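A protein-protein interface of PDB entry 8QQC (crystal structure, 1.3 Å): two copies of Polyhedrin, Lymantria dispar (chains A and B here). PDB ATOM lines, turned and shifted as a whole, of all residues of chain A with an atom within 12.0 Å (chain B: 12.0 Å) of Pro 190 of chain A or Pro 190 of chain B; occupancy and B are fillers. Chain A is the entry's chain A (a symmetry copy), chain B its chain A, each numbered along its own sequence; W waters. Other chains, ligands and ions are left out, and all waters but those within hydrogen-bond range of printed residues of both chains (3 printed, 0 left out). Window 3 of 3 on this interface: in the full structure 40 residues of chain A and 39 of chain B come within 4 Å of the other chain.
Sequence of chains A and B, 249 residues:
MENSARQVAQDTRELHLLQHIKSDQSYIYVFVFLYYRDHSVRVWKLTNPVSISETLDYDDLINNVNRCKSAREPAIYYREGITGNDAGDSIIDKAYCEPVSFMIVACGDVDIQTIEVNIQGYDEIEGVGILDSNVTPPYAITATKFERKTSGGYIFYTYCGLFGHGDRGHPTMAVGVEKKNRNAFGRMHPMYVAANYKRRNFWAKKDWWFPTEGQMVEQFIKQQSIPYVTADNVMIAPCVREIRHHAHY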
ATOM      1  N   GLU A 178     -18.763 -22.859 -39.193  1.00  0.00           N
ATOM      2  CA  GLU A 178     -19.369 -23.733 -38.197  1.00  0.00           C
ATOM      3  C   GLU A 178     -20.538 -24.491 -38.807  1.00  0.00           C
ATOM      4  O   GLU A 178     -21.145 -24.060 -39.791  1.00  0.00           O
ATOM      5  CB  GLU A 178     -19.894 -22.932 -36.999  1.00  0.00           C
ATOM      6  CG  GLU A 178     -18.849 -22.102 -36.284  1.00  0.00           C
ATOM      7  CD  GLU A 178     -19.431 -21.291 -35.136  1.00  0.00           C
ATOM      8  OE1 GLU A 178     -20.646 -21.407 -34.852  1.00  0.00           O
ATOM      9  OE2 GLU A 178     -18.667 -20.527 -34.518  1.00  0.00           O
ATOM     10  N   ASN A 181     -26.424 -24.617 -36.121  1.00  0.00           N
ATOM     11  CA  ASN A 181     -27.118 -25.090 -34.929  1.00  0.00           C
ATOM     12  C   ASN A 181     -28.440 -24.344 -34.832  1.00  0.00           C
ATOM     13  O   ASN A 181     -28.465 -23.154 -34.500  1.00  0.00           O
ATOM     14  CB  ASN A 181     -26.270 -24.858 -33.682  1.00  0.00           C
ATOM     15  CG  ASN A 181     -26.785 -25.631 -32.486  1.00  0.00           C
ATOM     16  OD1 ASN A 181     -27.935 -26.077 -32.469  1.00  0.00           O
ATOM     17  ND2 ASN A 181     -25.937 -25.799 -31.481  1.00  0.00           N
ATOM     18  N   ASN A 183     -30.777 -24.913 -32.716  1.00  0.00           N
ATOM     19  CA  ASN A 183     -31.297 -24.959 -31.358  1.00  0.00           C
ATOM     20  C   ASN A 183     -30.196 -24.483 -30.422  1.00  0.00           C
ATOM     21  O   ASN A 183     -29.195 -23.912 -30.864  1.00  0.00           O
ATOM     22  CB  ASN A 183     -31.907 -26.333 -31.060  1.00  0.00           C
ATOM     23  CG  ASN A 183     -33.165 -26.577 -31.859  1.00  0.00           C
ATOM     24  OD1 ASN A 183     -34.214 -26.016 -31.553  1.00  0.00           O
ATOM     25  ND2 ASN A 183     -33.062 -27.391 -32.904  1.00  0.00           N
ATOM     26  N   ALA A 184     -30.376 -24.705 -29.118  1.00  0.00           N
ATOM     27  CA  ALA A 184     -29.585 -23.973 -28.138  1.00  0.00           C
ATOM     28  C   ALA A 184     -28.418 -24.748 -27.551  1.00  0.00           C
ATOM     29  O   ALA A 184     -27.520 -24.120 -26.980  1.00  0.00           O
ATOM     30  CB  ALA A 184     -30.471 -23.485 -26.990  1.00  0.00           C
ATOM     31  N   PHE A 185     -28.413 -26.076 -27.638  1.00  0.00           N
ATOM     32  CA  PHE A 185     -27.337 -26.848 -27.027  1.00  0.00           C
ATOM     33  C   PHE A 185     -26.112 -26.770 -27.927  1.00  0.00           C
ATOM     34  O   PHE A 185     -26.100 -27.339 -29.023  1.00  0.00           O
ATOM     35  CB  PHE A 185     -27.753 -28.298 -26.802  1.00  0.00           C
ATOM     36  CG  PHE A 185     -26.693 -29.116 -26.127  1.00  0.00           C
ATOM     37  CD1 PHE A 185     -26.361 -28.877 -24.800  1.00  0.00           C
ATOM     38  CD2 PHE A 185     -25.994 -30.088 -26.824  1.00  0.00           C
ATOM     39  CE1 PHE A 185     -25.370 -29.614 -24.171  1.00  0.00           C
ATOM     40  CE2 PHE A 185     -24.996 -30.821 -26.203  1.00  0.00           C
ATOM     41  CZ  PHE A 185     -24.687 -30.585 -24.876  1.00  0.00           C
ATOM     42  N   GLY A 186     -25.081 -26.069 -27.467  1.00  0.00           N
ATOM     43  CA  GLY A 186     -23.930 -25.822 -28.316  1.00  0.00           C
ATOM     44  C   GLY A 186     -23.127 -27.087 -28.561  1.00  0.00           C
ATOM     45  O   GLY A 186     -22.986 -27.944 -27.687  1.00  0.00           O
ATOM     46  N   ARG A 187     -22.588 -27.202 -29.771  1.00  0.00           N
ATOM     47  CA  ARG A 187     -21.769 -28.366 -30.078  1.00  0.00           C
ATOM     48  C   ARG A 187     -20.409 -28.307 -29.398  1.00  0.00           C
ATOM     49  O   ARG A 187     -19.692 -29.315 -29.378  1.00  0.00           O
ATOM     50  CB  ARG A 187     -21.713 -28.582 -31.593  1.00  0.00           C
ATOM     51  CG  ARG A 187     -23.118 -28.751 -32.168  1.00  0.00           C
ATOM     52  CD  ARG A 187     -23.192 -29.686 -33.355  1.00  0.00           C
ATOM     53  NE  ARG A 187     -24.579 -29.941 -33.734  1.00  0.00           N
ATOM     54  CZ  ARG A 187     -25.332 -29.118 -34.454  1.00  0.00           C
ATOM     55  NH1 ARG A 187     -24.873 -27.954 -34.882  1.00  0.00           N
ATOM     56  NH2 ARG A 187     -26.577 -29.476 -34.758  1.00  0.00           N
ATOM     57  N   MET A 188     -20.053 -27.165 -28.806  1.00  0.00           N
ATOM     58  CA  MET A 188     -18.951 -27.097 -27.854  1.00  0.00           C
ATOM     59  C   MET A 188     -19.382 -26.694 -26.448  1.00  0.00           C
ATOM     60  O   MET A 188     -18.571 -26.167 -25.681  1.00  0.00           O
ATOM     61  CB  MET A 188     -17.741 -26.307 -28.354  1.00  0.00           C
ATOM     62  CG  MET A 188     -17.371 -26.599 -29.785  1.00  0.00           C
ATOM     63  SD  MET A 188     -16.223 -27.979 -29.635  1.00  0.00           S
ATOM     64  CE  MET A 188     -14.717 -27.107 -29.222  1.00  0.00           C
ATOM     65  N   HIS A 189     -20.637 -26.955 -26.092  1.00  0.00           N
ATOM     66  CA  HIS A 189     -21.057 -26.889 -24.703  1.00  0.00           C
ATOM     67  C   HIS A 189     -20.209 -27.857 -23.875  1.00  0.00           C
ATOM     68  O   HIS A 189     -19.750 -28.879 -24.394  1.00  0.00           O
ATOM     69  CB  HIS A 189     -22.519 -27.310 -24.618  1.00  0.00           C
ATOM     70  CG  HIS A 189     -23.100 -27.209 -23.245  1.00  0.00           C
ATOM     71  ND1 HIS A 189     -22.930 -28.187 -22.288  1.00  0.00           N
ATOM     72  CD2 HIS A 189     -23.848 -26.241 -22.667  1.00  0.00           C
ATOM     73  CE1 HIS A 189     -23.543 -27.821 -21.177  1.00  0.00           C
ATOM     74  NE2 HIS A 189     -24.109 -26.645 -21.380  1.00  0.00           N
ATOM     75  N   PRO A 190     -19.974 -27.554 -22.585  1.00  0.00           N
ATOM     76  CA  PRO A 190     -19.133 -28.439 -21.752  1.00  0.00           C
ATOM     77  C   PRO A 190     -19.474 -29.924 -21.799  1.00  0.00           C
ATOM     78  O   PRO A 190     -18.566 -30.760 -21.708  1.00  0.00           O
ATOM     79  CB  PRO A 190     -19.322 -27.854 -20.346  1.00  0.00           C
ATOM     80  CG  PRO A 190     -19.453 -26.404 -20.604  1.00  0.00           C
ATOM     81  CD  PRO A 190     -20.278 -26.295 -21.878  1.00  0.00           C
ATOM     82  N   MET A 191     -20.747 -30.285 -21.951  1.00  0.00           N
ATOM     83  CA  MET A 191     -21.146 -31.685 -21.993  1.00  0.00           C
ATOM     84  C   MET A 191     -20.850 -32.335 -23.336  1.00  0.00           C
ATOM     85  O   MET A 191     -20.995 -33.556 -23.463  1.00  0.00           O
ATOM     86  CB  MET A 191     -22.640 -31.778 -21.688  1.00  0.00           C
ATOM     87  CG  MET A 191     -22.973 -31.496 -20.236  1.00  0.00           C
ATOM     88  SD  MET A 191     -24.655 -31.975 -19.832  1.00  0.00           S
ATOM     89  CE  MET A 191     -24.756 -31.422 -18.128  1.00  0.00           C
ATOM     90  N   TYR A 192     -20.419 -31.552 -24.328  1.00  0.00           N
ATOM     91  CA  TYR A 192     -20.176 -32.037 -25.675  1.00  0.00           C
ATOM     92  C   TYR A 192     -18.759 -31.729 -26.138  1.00  0.00           C
ATOM     93  O   TYR A 192     -18.221 -32.474 -26.965  1.00  0.00           O
ATOM     94  CB  TYR A 192     -21.186 -31.373 -26.635  1.00  0.00           C
ATOM     95  CG  TYR A 192     -21.584 -32.141 -27.890  1.00  0.00           C
ATOM     96  CD1 TYR A 192     -20.906 -33.280 -28.304  1.00  0.00           C
ATOM     97  CD2 TYR A 192     -22.694 -31.738 -28.630  1.00  0.00           C
ATOM     98  CE1 TYR A 192     -21.299 -33.973 -29.441  1.00  0.00           C
ATOM     99  CE2 TYR A 192     -23.097 -32.428 -29.764  1.00  0.00           C
ATOM    100  CZ  TYR A 192     -22.395 -33.544 -30.165  1.00  0.00           C
ATOM    101  OH  TYR A 192     -22.797 -34.236 -31.288  1.00  0.00           O
ATOM    102  N   VAL A 193     -18.122 -30.698 -25.567  1.00  0.00           N
ATOM    103  CA  VAL A 193     -16.881 -30.141 -26.116  1.00  0.00           C
ATOM    104  C   VAL A 193     -15.809 -31.208 -26.324  1.00  0.00           C
ATOM    105  O   VAL A 193     -15.156 -31.253 -27.373  1.00  0.00           O
ATOM    106  CB  VAL A 193     -16.384 -28.962 -25.257  1.00  0.00           C
ATOM    107  CG1 VAL A 193     -16.130 -29.390 -23.808  1.00  0.00           C
ATOM    108  CG2 VAL A 193     -15.119 -28.344 -25.855  1.00  0.00           C
ATOM    109  N   ALA A 194     -15.602 -32.080 -25.335  1.00  0.00           N
ATOM    110  CA  ALA A 194     -14.492 -33.027 -25.436  1.00  0.00           C
ATOM    111  C   ALA A 194     -14.668 -33.978 -26.611  1.00  0.00           C
ATOM    112  O   ALA A 194     -13.685 -34.349 -27.268  1.00  0.00           O
ATOM    113  CB  ALA A 194     -14.324 -33.805 -24.132  1.00  0.00           C
ATOM    114  N   ALA A 195     -15.911 -34.352 -26.914  1.00  0.00           N
ATOM    115  CA  ALA A 195     -16.159 -35.278 -28.011  1.00  0.00           C
ATOM    116  C   ALA A 195     -15.877 -34.633 -29.356  1.00  0.00           C
ATOM    117  O   ALA A 195     -15.432 -35.311 -30.288  1.00  0.00           O
ATOM    118  CB  ALA A 195     -17.600 -35.778 -27.952  1.00  0.00           C
ATOM    119  N   ASN A 196     -16.128 -33.331 -29.483  1.00  0.00           N
ATOM    120  CA  ASN A 196     -15.832 -32.661 -30.737  1.00  0.00           C
ATOM    121  C   ASN A 196     -14.375 -32.215 -30.809  1.00  0.00           C
ATOM    122  O   ASN A 196     -13.786 -32.221 -31.893  1.00  0.00           O
ATOM    123  CB  ASN A 196     -16.810 -31.514 -30.991  1.00  0.00           C
ATOM    124  CG  ASN A 196     -18.139 -32.004 -31.522  1.00  0.00           C
ATOM    125  OD1 ASN A 196     -19.204 -31.704 -30.977  1.00  0.00           O
ATOM    126  ND2 ASN A 196     -18.075 -32.823 -32.562  1.00  0.00           N
ATOM    127  N   TYR A 197     -13.782 -31.856 -29.669  1.00  0.00           N
ATOM    128  CA  TYR A 197     -12.358 -31.536 -29.622  1.00  0.00           C
ATOM    129  C   TYR A 197     -11.514 -32.723 -30.070  1.00  0.00           C
ATOM    130  O   TYR A 197     -10.491 -32.551 -30.745  1.00  0.00           O
ATOM    131  CB  TYR A 197     -11.998 -31.142 -28.193  1.00  0.00           C
ATOM    132  CG  TYR A 197     -10.609 -30.581 -27.988  1.00  0.00           C
ATOM    133  CD1 TYR A 197     -10.186 -29.436 -28.655  1.00  0.00           C
ATOM    134  CD2 TYR A 197      -9.732 -31.176 -27.089  1.00  0.00           C
ATOM    135  CE1 TYR A 197      -8.917 -28.913 -28.441  1.00  0.00           C
ATOM    136  CE2 TYR A 197      -8.466 -30.662 -26.870  1.00  0.00           C
ATOM    137  CZ  TYR A 197      -8.063 -29.537 -27.550  1.00  0.00           C
ATOM    138  OH  TYR A 197      -6.806 -29.046 -27.304  1.00  0.00           O
ATOM    139  N   LYS A 198     -11.937 -33.937 -29.703  1.00  0.00           N
ATOM    140  CA  LYS A 198     -11.265 -35.153 -30.146  1.00  0.00           C
ATOM    141  C   LYS A 198     -11.314 -35.307 -31.657  1.00  0.00           C
ATOM    142  O   LYS A 198     -10.523 -36.067 -32.221  1.00  0.00           O
ATOM    143  CB  LYS A 198     -11.938 -36.366 -29.494  1.00  0.00           C
ATOM    144  CG  LYS A 198     -11.115 -37.651 -29.531  1.00  0.00           C
ATOM    145  CD  LYS A 198     -11.991 -38.862 -29.268  1.00  0.00           C
ATOM    146  CE  LYS A 198     -12.804 -39.235 -30.501  1.00  0.00           C
ATOM    147  NZ  LYS A 198     -13.724 -40.369 -30.220  1.00  0.00           N
ATOM    148  N   ASN B 181      -5.960 -12.081 -20.620  1.00  0.00           N
ATOM    149  CA  ASN B 181      -7.331 -11.749 -20.253  1.00  0.00           C
ATOM    150  C   ASN B 181      -7.296 -11.045 -18.905  1.00  0.00           C
ATOM    151  O   ASN B 181      -7.064 -11.683 -17.872  1.00  0.00           O
ATOM    152  CB  ASN B 181      -8.193 -13.007 -20.188  1.00  0.00           C
ATOM    153  CG  ASN B 181      -9.672 -12.687 -20.152  1.00  0.00           C
ATOM    154  OD1 ASN B 181     -10.069 -11.559 -19.848  1.00  0.00           O
ATOM    155  ND2 ASN B 181     -10.498 -13.674 -20.467  1.00  0.00           N
ATOM    156  N   ALA B 184     -12.802 -11.441 -16.445  1.00  0.00           N
ATOM    157  CA  ALA B 184     -13.215 -12.777 -16.038  1.00  0.00           C
ATOM    158  C   ALA B 184     -13.891 -13.595 -17.123  1.00  0.00           C
ATOM    159  O   ALA B 184     -13.973 -14.820 -16.974  1.00  0.00           O
ATOM    160  CB  ALA B 184     -14.151 -12.703 -14.829  1.00  0.00           C
ATOM    161  N   PHE B 185     -14.404 -12.972 -18.181  1.00  0.00           N
ATOM    162  CA  PHE B 185     -15.115 -13.727 -19.206  1.00  0.00           C
ATOM    163  C   PHE B 185     -14.091 -14.421 -20.093  1.00  0.00           C
ATOM    164  O   PHE B 185     -13.376 -13.768 -20.859  1.00  0.00           O
ATOM    165  CB  PHE B 185     -16.023 -12.822 -20.032  1.00  0.00           C
ATOM    166  CG  PHE B 185     -16.813 -13.568 -21.067  1.00  0.00           C
ATOM    167  CD1 PHE B 185     -17.823 -14.439 -20.684  1.00  0.00           C
ATOM    168  CD2 PHE B 185     -16.518 -13.441 -22.414  1.00  0.00           C
ATOM    169  CE1 PHE B 185     -18.548 -15.149 -21.629  1.00  0.00           C
ATOM    170  CE2 PHE B 185     -17.233 -14.153 -23.363  1.00  0.00           C
ATOM    171  CZ  PHE B 185     -18.249 -15.005 -22.969  1.00  0.00           C
ATOM    172  N   GLY B 186     -14.021 -15.745 -19.995  1.00  0.00           N
ATOM    173  CA  GLY B 186     -12.980 -16.474 -20.695  1.00  0.00           C
ATOM    174  C   GLY B 186     -13.198 -16.468 -22.198  1.00  0.00           C
ATOM    175  O   GLY B 186     -14.326 -16.524 -22.688  1.00  0.00           O
ATOM    176  N   ARG B 187     -12.097 -16.403 -22.940  1.00  0.00           N
ATOM    177  CA  ARG B 187     -12.213 -16.432 -24.391  1.00  0.00           C
ATOM    178  C   ARG B 187     -12.569 -17.817 -24.911  1.00  0.00           C
ATOM    179  O   ARG B 187     -12.920 -17.955 -26.089  1.00  0.00           O
ATOM    180  CB  ARG B 187     -10.964 -15.816 -25.028  1.00  0.00           C
ATOM    181  CG  ARG B 187     -10.755 -14.385 -24.537  1.00  0.00           C
ATOM    182  CD  ARG B 187     -10.135 -13.463 -25.565  1.00  0.00           C
ATOM    183  NE  ARG B 187     -10.135 -12.080 -25.094  1.00  0.00           N
ATOM    184  CZ  ARG B 187      -9.255 -11.570 -24.242  1.00  0.00           C
ATOM    185  NH1 ARG B 187      -8.287 -12.305 -23.720  1.00  0.00           N
ATOM    186  NH2 ARG B 187      -9.345 -10.284 -23.908  1.00  0.00           N
ATOM    187  N   MET B 188     -12.527 -18.839 -24.053  1.00  0.00           N
ATOM    188  CA  MET B 188     -13.161 -20.119 -24.344  1.00  0.00           C
ATOM    189  C   MET B 188     -14.290 -20.474 -23.382  1.00  0.00           C
ATOM    190  O   MET B 188     -14.604 -21.655 -23.207  1.00  0.00           O
ATOM    191  CB  MET B 188     -12.176 -21.271 -24.555  1.00  0.00           C
ATOM    192  CG  MET B 188     -10.986 -20.907 -25.403  1.00  0.00           C
ATOM    193  SD  MET B 188     -11.548 -21.276 -27.073  1.00  0.00           S
ATOM    194  CE  MET B 188     -11.285 -23.045 -27.123  1.00  0.00           C
ATOM    195  N   HIS B 189     -14.920 -19.470 -22.778  1.00  0.00           N
ATOM    196  CA  HIS B 189     -16.182 -19.676 -22.090  1.00  0.00           C
ATOM    197  C   HIS B 189     -17.207 -20.239 -23.076  1.00  0.00           C
ATOM    198  O   HIS B 189     -17.131 -19.960 -24.276  1.00  0.00           O
ATOM    199  CB  HIS B 189     -16.677 -18.331 -21.570  1.00  0.00           C
ATOM    200  CG  HIS B 189     -17.935 -18.416 -20.769  1.00  0.00           C
ATOM    201  ND1 HIS B 189     -19.186 -18.472 -21.346  1.00  0.00           N
ATOM    202  CD2 HIS B 189     -18.134 -18.458 -19.431  1.00  0.00           C
ATOM    203  CE1 HIS B 189     -20.101 -18.553 -20.397  1.00  0.00           C
ATOM    204  NE2 HIS B 189     -19.489 -18.545 -19.226  1.00  0.00           N
ATOM    205  N   PRO B 190     -18.172 -21.047 -22.600  1.00  0.00           N
ATOM    206  CA  PRO B 190     -19.166 -21.644 -23.516  1.00  0.00           C
ATOM    207  C   PRO B 190     -19.839 -20.682 -24.490  1.00  0.00           C
ATOM    208  O   PRO B 190     -20.145 -21.079 -25.622  1.00  0.00           O
ATOM    209  CB  PRO B 190     -20.176 -22.276 -22.550  1.00  0.00           C
ATOM    210  CG  PRO B 190     -19.326 -22.724 -21.426  1.00  0.00           C
ATOM    211  CD  PRO B 190     -18.285 -21.629 -21.247  1.00  0.00           C
ATOM    212  N   MET B 191     -20.067 -19.431 -24.100  1.00  0.00           N
ATOM    213  CA  MET B 191     -20.715 -18.463 -24.974  1.00  0.00           C
ATOM    214  C   MET B 191     -19.773 -17.911 -26.033  1.00  0.00           C
ATOM    215  O   MET B 191     -20.226 -17.198 -26.935  1.00  0.00           O
ATOM    216  CB  MET B 191     -21.264 -17.320 -24.119  1.00  0.00           C
ATOM    217  CG  MET B 191     -22.471 -17.718 -23.294  1.00  0.00           C
ATOM    218  SD  MET B 191     -23.309 -16.287 -22.604  1.00  0.00           S
ATOM    219  CE  MET B 191     -24.582 -17.087 -21.626  1.00  0.00           C
ATOM    220  N   TYR B 192     -18.482 -18.242 -25.954  1.00  0.00           N
ATOM    221  CA  TYR B 192     -17.471 -17.720 -26.857  1.00  0.00           C
ATOM    222  C   TYR B 192     -16.701 -18.837 -27.547  1.00  0.00           C
ATOM    223  O   TYR B 192     -16.216 -18.631 -28.666  1.00  0.00           O
ATOM    224  CB  TYR B 192     -16.490 -16.840 -26.053  1.00  0.00           C
ATOM    225  CG  TYR B 192     -15.789 -15.705 -26.789  1.00  0.00           C
ATOM    226  CD1 TYR B 192     -15.821 -15.590 -28.173  1.00  0.00           C
ATOM    227  CD2 TYR B 192     -15.134 -14.707 -26.068  1.00  0.00           C
ATOM    228  CE1 TYR B 192     -15.190 -14.536 -28.819  1.00  0.00           C
ATOM    229  CE2 TYR B 192     -14.505 -13.649 -26.705  1.00  0.00           C
ATOM    230  CZ  TYR B 192     -14.535 -13.569 -28.080  1.00  0.00           C
ATOM    231  OH  TYR B 192     -13.916 -12.514 -28.716  1.00  0.00           O
ATOM    232  N   VAL B 193     -16.645 -20.029 -26.940  1.00  0.00           N
ATOM    233  CA  VAL B 193     -15.715 -21.083 -27.363  1.00  0.00           C
ATOM    234  C   VAL B 193     -15.835 -21.398 -28.852  1.00  0.00           C
ATOM    235  O   VAL B 193     -14.827 -21.518 -29.557  1.00  0.00           O
ATOM    236  CB  VAL B 193     -15.871 -22.336 -26.479  1.00  0.00           C
ATOM    237  CG1 VAL B 193     -17.298 -22.890 -26.533  1.00  0.00           C
ATOM    238  CG2 VAL B 193     -14.868 -23.418 -26.883  1.00  0.00           C
ATOM    239  N   ALA B 194     -17.063 -21.543 -29.358  1.00  0.00           N
ATOM    240  CA  ALA B 194     -17.217 -21.983 -30.745  1.00  0.00           C
ATOM    241  C   ALA B 194     -16.631 -20.975 -31.723  1.00  0.00           C
ATOM    242  O   ALA B 194     -16.060 -21.363 -32.753  1.00  0.00           O
ATOM    243  CB  ALA B 194     -18.686 -22.256 -31.065  1.00  0.00           C
ATOM    244  N   ALA B 195     -16.728 -19.685 -31.404  1.00  0.00           N
ATOM    245  CA  ALA B 195     -16.212 -18.659 -32.300  1.00  0.00           C
ATOM    246  C   ALA B 195     -14.695 -18.677 -32.347  1.00  0.00           C
ATOM    247  O   ALA B 195     -14.103 -18.387 -33.393  1.00  0.00           O
ATOM    248  CB  ALA B 195     -16.715 -17.286 -31.862  1.00  0.00           C
ATOM    249  N   ASN B 196     -14.044 -19.009 -31.233  1.00  0.00           N
ATOM    250  CA  ASN B 196     -12.594 -19.083 -31.243  1.00  0.00           C
ATOM    251  C   ASN B 196     -12.101 -20.440 -31.735  1.00  0.00           C
ATOM    252  O   ASN B 196     -11.053 -20.512 -32.385  1.00  0.00           O
ATOM    253  CB  ASN B 196     -12.017 -18.708 -29.879  1.00  0.00           C
ATOM    254  CG  ASN B 196     -11.977 -17.211 -29.666  1.00  0.00           C
ATOM    255  OD1 ASN B 196     -12.494 -16.684 -28.679  1.00  0.00           O
ATOM    256  ND2 ASN B 196     -11.414 -16.508 -30.639  1.00  0.00           N
ATOM    257  N   TYR B 197     -12.852 -21.507 -31.460  1.00  0.00           N
ATOM    258  CA  TYR B 197     -12.524 -22.826 -31.997  1.00  0.00           C
ATOM    259  C   TYR B 197     -12.523 -22.811 -33.521  1.00  0.00           C
ATOM    260  O   TYR B 197     -11.688 -23.468 -34.157  1.00  0.00           O
ATOM    261  CB  TYR B 197     -13.552 -23.827 -31.480  1.00  0.00           C
ATOM    262  CG  TYR B 197     -13.262 -25.283 -31.765  1.00  0.00           C
ATOM    263  CD1 TYR B 197     -12.098 -25.892 -31.307  1.00  0.00           C
ATOM    264  CD2 TYR B 197     -14.180 -26.063 -32.458  1.00  0.00           C
ATOM    265  CE1 TYR B 197     -11.852 -27.237 -31.551  1.00  0.00           C
ATOM    266  CE2 TYR B 197     -13.943 -27.404 -32.706  1.00  0.00           C
ATOM    267  CZ  TYR B 197     -12.779 -27.983 -32.256  1.00  0.00           C
ATOM    268  OH  TYR B 197     -12.578 -29.316 -32.510  1.00  0.00           O
ATOM    269  N   LYS B 198     -13.452 -22.060 -34.119  1.00  0.00           N
ATOM    270  CA  LYS B 198     -13.495 -21.895 -35.567  1.00  0.00           C
ATOM    271  C   LYS B 198     -12.239 -21.223 -36.097  1.00  0.00           C
ATOM    272  O   LYS B 198     -11.953 -21.315 -37.293  1.00  0.00           O
ATOM    273  CB  LYS B 198     -14.716 -21.048 -35.941  1.00  0.00           C
ATOM    274  CG  LYS B 198     -15.123 -21.126 -37.411  1.00  0.00           C
ATOM    275  CD  LYS B 198     -16.032 -19.968 -37.782  1.00  0.00           C
ATOM    276  CE  LYS B 198     -15.240 -18.682 -37.972  1.00  0.00           C
ATOM    277  NZ  LYS B 198     -16.138 -17.530 -38.254  1.00  0.00           N
HETATM  278  O   HOH W   1     -19.944 -19.486 -32.588  1.00  0.00           O
HETATM  279  O   HOH W   2     -14.386 -30.565 -34.102  1.00  0.00           O
HETATM  280  O   HOH W   3     -21.266 -23.592 -25.691  1.00  0.00           O
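Of the 16 printed residues of chain B, 6 touch a printed residue of chain A. Hydrophobic or aromatic side chains of chain B that line the printed part of chain A: Pro 190, Val 193, Ala 194 and Tyr 197. Of the 18 printed residues of chain A, 5 touch a printed residue of chain B. Hydrophobic or aromatic side chains of chain A within 4 Å of the printed part of chain B: Met 188, Pro 190 and Tyr 197. Among the printed residues, no Asp or Glu carboxylate lies within 4 Å of a Lys or Arg side-chain nitrogen of the other chain.
The backbone carbonyl oxygen (O) of Ala 194 of chain B sits close to the side-chain carboxylate (OE2) of Glu 178 of chain A, 3.3 Å away. The side-chain hydroxyl (OH) of Tyr 197 of chain B lies within hydrogen-bond range of the backbone carbonyl oxygen (O) of Asn 196 of chain A, at 3.2 Å.
No residue of chain B comes within 4 Å of Gly 186 of chain A. Val 193 of chain A touches none of the printed residues of chain B. Gly 186 of chain B touches none of the printed residues of chain A. No residue of chain A comes within 4 Å of His 189 of chain B. No residue of chain A comes within 4 Å of Met 191 of chain B. Of chain A, only Met 188 (3.6 Å) comes within 4 Å of Val 193 of chain B. Of the printed residues of chain A, Ala 195 of chain B touches Glu 178 (3.8 Å). Printed residues of chain A within 4 Å of Ala 194 of chain B: Glu 178. Of the printed residues of chain B, Tyr 197 of chain A touches Tyr 197. Of the printed residues of chain B, Met 188 of chain A touches Val 193 and Tyr 197. The nearest residue of chain B that does not touch Pro 190 of chain A is Val 193 of chain B (6.5 Å).
Met 188 of chain A touches Tyr 197 of chain B, but with the chains exchanged Tyr 197 of chain A does not touch Met 188 of chain B (6.5 Å). Pro 190 of chain B touches its own counterpart, Pro 190 of chain A. Asn 196 of chain A touches Tyr 197 of chain B, but with the chains exchanged Tyr 197 of chain A does not touch Asn 196 of chain B (9.5 Å). Tyr 197 of chain A touches its own counterpart, Tyr 197 of chain B. Of the 8 pairs that touch across the chains among the printed residues, 2 have their exchanged pair printed and touching as well.
The side-chain amide oxygen (OD1) of Asn 196 of chain A lies close to the backbone carbonyl oxygen (O) of Arg 187 of chain A, at 2.9 Å.
Glu 178 of chain A touches Ala 195 of chain B (OE2 to N, 3.8 Å). Lys 198 of chain B touches Glu 178 of chain A. O of Met 188 of chain A touches CG1 of Val 193 of chain B, 3.6 Å away. Met 188 of chain A touches Tyr 197 of chain B. Pro 190 of chain A touches Pro 190 of chain B (CD to CG, 3.7 Å). Tyr 197 of chain A touches Tyr 197 of chain B.
Water W1 lies within hydrogen-bond range of OE2 of Glu 178 of chain A (2.5 Å) and N of Ala 195 of chain B (3.4 Å). Water W2 bridges OH of Tyr 197 of chain B and O of Asn 196 of chain A. Water W3 bridges O of Pro 190 of chain B (2.8 Å) and N of His 189 of chain A (3.4 Å).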
